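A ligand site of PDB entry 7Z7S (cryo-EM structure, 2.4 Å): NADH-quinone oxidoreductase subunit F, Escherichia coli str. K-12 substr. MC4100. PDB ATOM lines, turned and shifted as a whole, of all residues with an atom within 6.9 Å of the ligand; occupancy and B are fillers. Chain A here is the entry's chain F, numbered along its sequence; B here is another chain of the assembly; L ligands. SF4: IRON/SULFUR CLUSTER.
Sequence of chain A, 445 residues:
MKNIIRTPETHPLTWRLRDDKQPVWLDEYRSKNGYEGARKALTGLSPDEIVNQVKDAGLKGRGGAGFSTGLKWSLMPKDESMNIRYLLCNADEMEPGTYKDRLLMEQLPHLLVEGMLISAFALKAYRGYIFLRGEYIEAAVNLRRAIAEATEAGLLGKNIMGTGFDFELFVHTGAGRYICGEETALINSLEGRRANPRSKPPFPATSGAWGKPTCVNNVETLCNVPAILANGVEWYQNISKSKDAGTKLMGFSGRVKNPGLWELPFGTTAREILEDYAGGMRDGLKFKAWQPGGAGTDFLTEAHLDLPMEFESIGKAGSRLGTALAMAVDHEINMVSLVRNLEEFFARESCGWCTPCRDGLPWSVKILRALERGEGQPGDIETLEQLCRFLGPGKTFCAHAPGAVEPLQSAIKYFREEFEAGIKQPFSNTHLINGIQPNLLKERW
SG of Cys 357 is bound to FE2 of the ligand. The backbone NH (N) of Cys 354 lies close to a sulfur (S3) of the ligand, at 3.3 Å. The side-chain sulfur of Cys 354 binds an iron atom (FE1) of the ligand (2.3 Å). The side-chain sulfur (SG) of Cys 398 binds an iron atom (FE3) of the ligand (2.3 Å). The backbone NH of Cys 351 lies close to a sulfur (S1) of the ligand, at 3.5 Å. An iron atom (FE4) of the ligand is bound by the side-chain sulfur (SG) of Cys 351 (2.3 Å). N of Trp 353 sits close to S3 of the ligand (3.3 Å). S3 of the ligand lies close to OG of Ser 350, 3.5 Å away. N of Gly 352 lies close to S3 of the ligand (3.6 Å).
The side-chain sulfur (SG) of Cys 357 lies close to the side-chain hydroxyl (OG) of Ser 350, 3.2 Å away. The side-chain sulfur (SG) of Cys 398 sits close to the backbone NH (N) of His 400. The backbone carbonyl oxygen of Cys 398 lies within hydrogen-bond range of the side-chain hydroxyl of Thr 396 (2.6 Å). The side-chain sulfur (SG) of Cys 351 lies close to the backbone NH (N) of Trp 353 (3.4 Å). ND2 of Asn 196 lies close to SG of Cys 351, at 3.2 Å. The backbone carbonyl oxygen (O) of Trp 353 sits at hydrogen-bond distance from the guanidinium group (NH1) of Arg 358 (3.4 Å). O of Gly 352 sits at hydrogen-bond distance from NH1 of Arg 358, at 3.2 Å. The backbone carbonyl oxygen of Thr 396 is in hydrogen-bond range of the guanidinium group of Arg 46 of chain B.
CD1 of Ile 179 touches S1 of the ligand, at 3.7 Å. Pro 197 touches the ligand. Thr 396 touches the ligand. Phe 397 touches the ligand (CB to S2, 3.6 Å). His 400 touches the ligand (CB to S1, 3.6 Å). N of Ala 401 touches S4 of the ligand (3.97 Å). Hydrophobic or aromatic side chains that line the ligand: Ile 179, Pro 197, Trp 353, Phe 397 and His 400. 13 residues have an atom within 4 Å of the ligand: Ile 179, Pro 197, Ser 350, Cys 351, Gly 352, Trp 353, Cys 354, Cys 357, Thr 396, Phe 397, Cys 398, His 400 and Ala 401. The nearest printed residue that does not touch the ligand is Arg 358 (4.4 Å).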
ATOM      1  N   ILE A 179      23.713  16.841 -18.298  1.00  0.00           N
ATOM      2  CA  ILE A 179      23.985  15.871 -19.353  1.00  0.00           C
ATOM      3  C   ILE A 179      23.652  14.440 -18.927  1.00  0.00           C
ATOM      4  O   ILE A 179      23.464  13.578 -19.783  1.00  0.00           O
ATOM      5  CB  ILE A 179      25.445  15.996 -19.830  1.00  0.00           C
ATOM      6  CG1 ILE A 179      25.670  15.356 -21.198  1.00  0.00           C
ATOM      7  CG2 ILE A 179      26.407  15.402 -18.804  1.00  0.00           C
ATOM      8  CD1 ILE A 179      24.599  15.634 -22.208  1.00  0.00           C
ATOM      9  N   GLU A 182      20.628  12.704 -20.687  1.00  0.00           N
ATOM     10  CA  GLU A 182      20.825  12.042 -21.971  1.00  0.00           C
ATOM     11  C   GLU A 182      21.028  10.551 -21.727  1.00  0.00           C
ATOM     12  O   GLU A 182      21.793  10.166 -20.849  1.00  0.00           O
ATOM     13  CB  GLU A 182      22.026  12.635 -22.694  1.00  0.00           C
ATOM     14  CG  GLU A 182      21.969  12.551 -24.196  1.00  0.00           C
ATOM     15  CD  GLU A 182      22.506  11.257 -24.752  1.00  0.00           C
ATOM     16  OE1 GLU A 182      23.174  10.527 -24.012  1.00  0.00           O
ATOM     17  OE2 GLU A 182      22.246  10.980 -25.942  1.00  0.00           O
ATOM     18  N   ALA A 195      29.717  11.158 -17.103  1.00  0.00           N
ATOM     19  CA  ALA A 195      28.503  11.055 -17.905  1.00  0.00           C
ATOM     20  C   ALA A 195      28.696  11.640 -19.301  1.00  0.00           C
ATOM     21  O   ALA A 195      28.079  12.617 -19.699  1.00  0.00           O
ATOM     22  CB  ALA A 195      27.346  11.729 -17.183  1.00  0.00           C
ATOM     23  N   ASN A 196      29.595  11.009 -20.052  1.00  0.00           N
ATOM     24  CA  ASN A 196      29.613  11.356 -21.460  1.00  0.00           C
ATOM     25  C   ASN A 196      28.598  10.504 -22.204  1.00  0.00           C
ATOM     26  O   ASN A 196      28.405   9.334 -21.866  1.00  0.00           O
ATOM     27  CB  ASN A 196      30.999  11.129 -22.068  1.00  0.00           C
ATOM     28  CG  ASN A 196      32.080  11.901 -21.362  1.00  0.00           C
ATOM     29  OD1 ASN A 196      32.977  11.324 -20.771  1.00  0.00           O
ATOM     30  ND2 ASN A 196      31.997  13.220 -21.431  1.00  0.00           N
ATOM     31  N   PRO A 197      27.928  11.046 -23.221  1.00  0.00           N
ATOM     32  CA  PRO A 197      27.057  10.214 -24.045  1.00  0.00           C
ATOM     33  C   PRO A 197      27.867   9.274 -24.930  1.00  0.00           C
ATOM     34  O   PRO A 197      29.093   9.374 -25.047  1.00  0.00           O
ATOM     35  CB  PRO A 197      26.275  11.234 -24.872  1.00  0.00           C
ATOM     36  CG  PRO A 197      27.040  12.472 -24.798  1.00  0.00           C
ATOM     37  CD  PRO A 197      27.801  12.472 -23.529  1.00  0.00           C
ATOM     38  N   PHE A 346      23.780  26.391 -20.838  1.00  0.00           N
ATOM     39  CA  PHE A 346      24.105  25.342 -21.800  1.00  0.00           C
ATOM     40  C   PHE A 346      25.608  25.142 -21.947  1.00  0.00           C
ATOM     41  O   PHE A 346      26.051  24.006 -22.125  1.00  0.00           O
ATOM     42  CB  PHE A 346      23.480  25.661 -23.147  1.00  0.00           C
ATOM     43  CG  PHE A 346      22.049  25.273 -23.257  1.00  0.00           C
ATOM     44  CD1 PHE A 346      21.659  23.958 -23.051  1.00  0.00           C
ATOM     45  CD2 PHE A 346      21.075  26.206 -23.552  1.00  0.00           C
ATOM     46  CE1 PHE A 346      20.337  23.595 -23.148  1.00  0.00           C
ATOM     47  CE2 PHE A 346      19.754  25.843 -23.648  1.00  0.00           C
ATOM     48  CZ  PHE A 346      19.383  24.543 -23.442  1.00  0.00           C
ATOM     49  N   GLU A 349      26.939  23.381 -18.823  1.00  0.00           N
ATOM     50  CA  GLU A 349      26.454  22.017 -18.689  1.00  0.00           C
ATOM     51  C   GLU A 349      26.959  21.118 -19.804  1.00  0.00           C
ATOM     52  O   GLU A 349      26.506  19.982 -19.921  1.00  0.00           O
ATOM     53  CB  GLU A 349      24.924  22.002 -18.660  1.00  0.00           C
ATOM     54  CG  GLU A 349      24.357  22.470 -17.336  1.00  0.00           C
ATOM     55  CD  GLU A 349      25.021  21.810 -16.145  1.00  0.00           C
ATOM     56  OE1 GLU A 349      24.967  20.569 -16.043  1.00  0.00           O
ATOM     57  OE2 GLU A 349      25.593  22.538 -15.305  1.00  0.00           O
ATOM     58  N   SER A 350      27.873  21.617 -20.621  1.00  0.00           N
ATOM     59  CA  SER A 350      28.560  20.784 -21.604  1.00  0.00           C
ATOM     60  C   SER A 350      29.344  19.700 -20.883  1.00  0.00           C
ATOM     61  O   SER A 350      29.940  19.931 -19.833  1.00  0.00           O
ATOM     62  CB  SER A 350      29.488  21.646 -22.442  1.00  0.00           C
ATOM     63  OG  SER A 350      30.302  20.864 -23.298  1.00  0.00           O
ATOM     64  N   CYS A 351      29.318  18.490 -21.435  1.00  0.00           N
ATOM     65  CA  CYS A 351      30.116  17.428 -20.839  1.00  0.00           C
ATOM     66  C   CYS A 351      31.577  17.502 -21.241  1.00  0.00           C
ATOM     67  O   CYS A 351      32.408  16.861 -20.589  1.00  0.00           O
ATOM     68  CB  CYS A 351      29.524  16.059 -21.199  1.00  0.00           C
ATOM     69  SG  CYS A 351      30.056  15.370 -22.751  1.00  0.00           S
ATOM     70  N   GLY A 352      31.918  18.284 -22.254  1.00  0.00           N
ATOM     71  CA  GLY A 352      33.290  18.471 -22.669  1.00  0.00           C
ATOM     72  C   GLY A 352      33.818  17.437 -23.635  1.00  0.00           C
ATOM     73  O   GLY A 352      35.017  17.454 -23.915  1.00  0.00           O
ATOM     74  N   TRP A 353      32.982  16.538 -24.134  1.00  0.00           N
ATOM     75  CA  TRP A 353      33.461  15.496 -25.030  1.00  0.00           C
ATOM     76  C   TRP A 353      33.842  16.061 -26.394  1.00  0.00           C
ATOM     77  O   TRP A 353      34.905  15.751 -26.918  1.00  0.00           O
ATOM     78  CB  TRP A 353      32.397  14.414 -25.172  1.00  0.00           C
ATOM     79  CG  TRP A 353      32.728  13.312 -26.112  1.00  0.00           C
ATOM     80  CD1 TRP A 353      32.085  13.008 -27.265  1.00  0.00           C
ATOM     81  CD2 TRP A 353      33.768  12.343 -25.976  1.00  0.00           C
ATOM     82  NE1 TRP A 353      32.660  11.924 -27.864  1.00  0.00           N
ATOM     83  CE2 TRP A 353      33.693  11.489 -27.081  1.00  0.00           C
ATOM     84  CE3 TRP A 353      34.761  12.112 -25.021  1.00  0.00           C
ATOM     85  CZ2 TRP A 353      34.572  10.429 -27.277  1.00  0.00           C
ATOM     86  CZ3 TRP A 353      35.628  11.067 -25.206  1.00  0.00           C
ATOM     87  CH2 TRP A 353      35.528  10.238 -26.317  1.00  0.00           C
ATOM     88  N   CYS A 354      32.987  16.893 -26.978  1.00  0.00           N
ATOM     89  CA  CYS A 354      33.149  17.244 -28.377  1.00  0.00           C
ATOM     90  C   CYS A 354      33.343  18.745 -28.566  1.00  0.00           C
ATOM     91  O   CYS A 354      32.716  19.555 -27.874  1.00  0.00           O
ATOM     92  CB  CYS A 354      31.990  16.701 -29.220  1.00  0.00           C
ATOM     93  SG  CYS A 354      30.456  17.581 -29.220  1.00  0.00           S
ATOM     94  N   THR A 355      34.210  19.080 -29.524  1.00  0.00           N
ATOM     95  CA  THR A 355      34.680  20.446 -29.735  1.00  0.00           C
ATOM     96  C   THR A 355      33.596  21.496 -29.976  1.00  0.00           C
ATOM     97  O   THR A 355      33.661  22.549 -29.332  1.00  0.00           O
ATOM     98  CB  THR A 355      35.691  20.467 -30.886  1.00  0.00           C
ATOM     99  OG1 THR A 355      36.785  19.591 -30.589  1.00  0.00           O
ATOM    100  CG2 THR A 355      36.239  21.860 -31.110  1.00  0.00           C
ATOM    101  N   PRO A 356      32.598  21.304 -30.869  1.00  0.00           N
ATOM    102  CA  PRO A 356      31.670  22.421 -31.150  1.00  0.00           C
ATOM    103  C   PRO A 356      30.892  22.892 -29.939  1.00  0.00           C
ATOM    104  O   PRO A 356      30.867  24.082 -29.669  1.00  0.00           O
ATOM    105  CB  PRO A 356      30.738  21.841 -32.223  1.00  0.00           C
ATOM    106  CG  PRO A 356      31.488  20.747 -32.809  1.00  0.00           C
ATOM    107  CD  PRO A 356      32.194  20.139 -31.663  1.00  0.00           C
ATOM    108  N   CYS A 357      30.348  21.970 -29.147  1.00  0.00           N
ATOM    109  CA  CYS A 357      29.627  22.376 -27.949  1.00  0.00           C
ATOM    110  C   CYS A 357      30.570  22.984 -26.917  1.00  0.00           C
ATOM    111  O   CYS A 357      30.420  24.156 -26.550  1.00  0.00           O
ATOM    112  CB  CYS A 357      28.871  21.182 -27.397  1.00  0.00           C
ATOM    113  SG  CYS A 357      28.287  21.176 -25.714  1.00  0.00           S
ATOM    114  N   ARG A 358      31.631  22.247 -26.571  1.00  0.00           N
ATOM    115  CA  ARG A 358      32.529  22.613 -25.470  1.00  0.00           C
ATOM    116  C   ARG A 358      33.242  23.932 -25.722  1.00  0.00           C
ATOM    117  O   ARG A 358      33.465  24.713 -24.789  1.00  0.00           O
ATOM    118  CB  ARG A 358      33.540  21.484 -25.234  1.00  0.00           C
ATOM    119  CG  ARG A 358      34.866  21.914 -24.621  1.00  0.00           C
ATOM    120  CD  ARG A 358      35.881  20.809 -24.536  1.00  0.00           C
ATOM    121  NE  ARG A 358      36.787  20.868 -25.672  1.00  0.00           N
ATOM    122  CZ  ARG A 358      36.819  19.966 -26.642  1.00  0.00           C
ATOM    123  NH1 ARG A 358      36.076  18.884 -26.598  1.00  0.00           N
ATOM    124  NH2 ARG A 358      37.616  20.170 -27.688  1.00  0.00           N
ATOM    125  N   LEU A 361      29.928  26.983 -27.540  1.00  0.00           N
ATOM    126  CA  LEU A 361      28.980  27.593 -26.600  1.00  0.00           C
ATOM    127  C   LEU A 361      29.608  28.683 -25.727  1.00  0.00           C
ATOM    128  O   LEU A 361      28.938  29.717 -25.529  1.00  0.00           O
ATOM    129  CB  LEU A 361      28.308  26.497 -25.777  1.00  0.00           C
ATOM    130  CG  LEU A 361      27.331  25.625 -26.550  1.00  0.00           C
ATOM    131  CD1 LEU A 361      26.728  24.549 -25.654  1.00  0.00           C
ATOM    132  CD2 LEU A 361      26.243  26.481 -27.164  1.00  0.00           C
ATOM    133  N   THR A 396      27.530  17.853 -33.708  1.00  0.00           N
ATOM    134  CA  THR A 396      28.041  17.515 -32.395  1.00  0.00           C
ATOM    135  C   THR A 396      27.771  16.050 -32.075  1.00  0.00           C
ATOM    136  O   THR A 396      27.038  15.354 -32.790  1.00  0.00           O
ATOM    137  CB  THR A 396      27.428  18.415 -31.325  1.00  0.00           C
ATOM    138  OG1 THR A 396      26.008  18.201 -31.275  1.00  0.00           O
ATOM    139  CG2 THR A 396      27.696  19.857 -31.653  1.00  0.00           C
ATOM    140  N   PHE A 397      28.377  15.592 -30.991  1.00  0.00           N
ATOM    141  CA  PHE A 397      28.304  14.179 -30.642  1.00  0.00           C
ATOM    142  C   PHE A 397      26.928  13.795 -30.104  1.00  0.00           C
ATOM    143  O   PHE A 397      26.461  12.677 -30.351  1.00  0.00           O
ATOM    144  CB  PHE A 397      29.393  13.846 -29.638  1.00  0.00           C
ATOM    145  CG  PHE A 397      29.585  12.389 -29.405  1.00  0.00           C
ATOM    146  CD1 PHE A 397      30.310  11.623 -30.305  1.00  0.00           C
ATOM    147  CD2 PHE A 397      29.062  11.778 -28.283  1.00  0.00           C
ATOM    148  CE1 PHE A 397      30.497  10.284 -30.078  1.00  0.00           C
ATOM    149  CE2 PHE A 397      29.244  10.439 -28.070  1.00  0.00           C
ATOM    150  CZ  PHE A 397      29.971   9.696 -28.962  1.00  0.00           C
ATOM    151  N   CYS A 398      26.287  14.687 -29.369  1.00  0.00           N
ATOM    152  CA  CYS A 398      24.935  14.451 -28.863  1.00  0.00           C
ATOM    153  C   CYS A 398      24.080  15.680 -29.125  1.00  0.00           C
ATOM    154  O   CYS A 398      24.527  16.656 -29.732  1.00  0.00           O
ATOM    155  CB  CYS A 398      24.965  14.072 -27.374  1.00  0.00           C
ATOM    156  SG  CYS A 398      24.860  15.430 -26.206  1.00  0.00           S
ATOM    157  N   ALA A 399      22.841  15.638 -28.658  1.00  0.00           N
ATOM    158  CA  ALA A 399      21.846  16.645 -28.983  1.00  0.00           C
ATOM    159  C   ALA A 399      21.798  17.796 -28.000  1.00  0.00           C
ATOM    160  O   ALA A 399      20.873  18.612 -28.064  1.00  0.00           O
ATOM    161  CB  ALA A 399      20.466  15.996 -29.089  1.00  0.00           C
ATOM    162  N   HIS A 400      22.757  17.885 -27.078  1.00  0.00           N
ATOM    163  CA  HIS A 400      22.781  18.980 -26.113  1.00  0.00           C
ATOM    164  C   HIS A 400      23.005  20.325 -26.799  1.00  0.00           C
ATOM    165  O   HIS A 400      22.318  21.303 -26.506  1.00  0.00           O
ATOM    166  CB  HIS A 400      23.858  18.712 -25.067  1.00  0.00           C
ATOM    167  CG  HIS A 400      24.233  19.907 -24.263  1.00  0.00           C
ATOM    168  ND1 HIS A 400      23.524  20.316 -23.166  1.00  0.00           N
ATOM    169  CD2 HIS A 400      25.254  20.787 -24.398  1.00  0.00           C
ATOM    170  CE1 HIS A 400      24.082  21.398 -22.644  1.00  0.00           C
ATOM    171  NE2 HIS A 400      25.139  21.694 -23.376  1.00  0.00           N
ATOM    172  N   ALA A 401      23.945  20.384 -27.738  1.00  0.00           N
ATOM    173  CA  ALA A 401      24.259  21.629 -28.427  1.00  0.00           C
ATOM    174  C   ALA A 401      23.227  22.070 -29.480  1.00  0.00           C
ATOM    175  O   ALA A 401      23.028  23.289 -29.613  1.00  0.00           O
ATOM    176  CB  ALA A 401      25.645  21.527 -29.072  1.00  0.00           C
ATOM    177  N   PRO A 402      22.581  21.189 -30.257  1.00  0.00           N
ATOM    178  CA  PRO A 402      21.443  21.665 -31.063  1.00  0.00           C
ATOM    179  C   PRO A 402      20.329  22.282 -30.244  1.00  0.00           C
ATOM    180  O   PRO A 402      19.762  23.325 -30.622  1.00  0.00           O
ATOM    181  CB  PRO A 402      20.979  20.397 -31.791  1.00  0.00           C
ATOM    182  CG  PRO A 402      22.157  19.581 -31.898  1.00  0.00           C
ATOM    183  CD  PRO A 402      22.957  19.814 -30.666  1.00  0.00           C
ATOM    184  N   ALA B  44      35.147  12.319 -31.102  1.00  0.00           N
ATOM    185  CA  ALA B  44      35.206  13.402 -30.119  1.00  0.00           C
ATOM    186  C   ALA B  44      35.475  14.754 -30.784  1.00  0.00           C
ATOM    187  O   ALA B  44      34.674  15.679 -30.645  1.00  0.00           O
ATOM    188  CB  ALA B  44      36.263  13.106 -29.059  1.00  0.00           C
ATOM    189  N   ARG B  46      35.401  16.083 -33.713  1.00  0.00           N
ATOM    190  CA  ARG B  46      34.521  16.525 -34.797  1.00  0.00           C
ATOM    191  C   ARG B  46      35.286  17.201 -35.944  1.00  0.00           C
ATOM    192  O   ARG B  46      34.700  17.909 -36.751  1.00  0.00           O
ATOM    193  CB  ARG B  46      33.397  17.438 -34.305  1.00  0.00           C
ATOM    194  CG  ARG B  46      32.701  16.945 -33.040  1.00  0.00           C
ATOM    195  CD  ARG B  46      32.183  15.550 -33.156  1.00  0.00           C
ATOM    196  NE  ARG B  46      30.953  15.460 -33.922  1.00  0.00           N
ATOM    197  CZ  ARG B  46      30.263  14.335 -34.068  1.00  0.00           C
ATOM    198  NH1 ARG B  46      30.669  13.215 -33.514  1.00  0.00           N
ATOM    199  NH2 ARG B  46      29.162  14.349 -34.805  1.00  0.00           N
ATOM    200  N   HIS B 176      33.080  20.900 -18.624  1.00  0.00           N
ATOM    201  CA  HIS B 176      32.802  21.406 -19.965  1.00  0.00           C
ATOM    202  C   HIS B 176      33.973  21.929 -20.776  1.00  0.00           C
ATOM    203  O   HIS B 176      34.535  21.185 -21.573  1.00  0.00           O
ATOM    204  CB  HIS B 176      31.837  22.571 -19.724  1.00  0.00           C
ATOM    205  CG  HIS B 176      32.056  23.220 -18.392  1.00  0.00           C
ATOM    206  ND1 HIS B 176      33.002  24.212 -18.201  1.00  0.00           N
ATOM    207  CD2 HIS B 176      31.515  22.994 -17.182  1.00  0.00           C
ATOM    208  CE1 HIS B 176      33.006  24.578 -16.935  1.00  0.00           C
ATOM    209  NE2 HIS B 176      32.120  23.848 -16.286  1.00  0.00           N
HETATM  210 FE1  SF4 L   1      29.293  17.214 -27.243  1.00  0.00          FE
HETATM  211 FE2  SF4 L   1      28.205  18.875 -25.579  1.00  0.00          FE
HETATM  212 FE3  SF4 L   1      26.923  16.490 -26.033  1.00  0.00          FE
HETATM  213 FE4  SF4 L   1      29.115  16.506 -24.549  1.00  0.00          FE
HETATM  214  S1  SF4 L   1      27.146  17.559 -24.006  1.00  0.00           S
HETATM  215  S2  SF4 L   1      28.765  15.141 -26.374  1.00  0.00           S
HETATM  216  S3  SF4 L   1      30.395  18.168 -25.466  1.00  0.00           S
HETATM  217  S4  SF4 L   1      27.236  18.176 -27.554  1.00  0.00           S
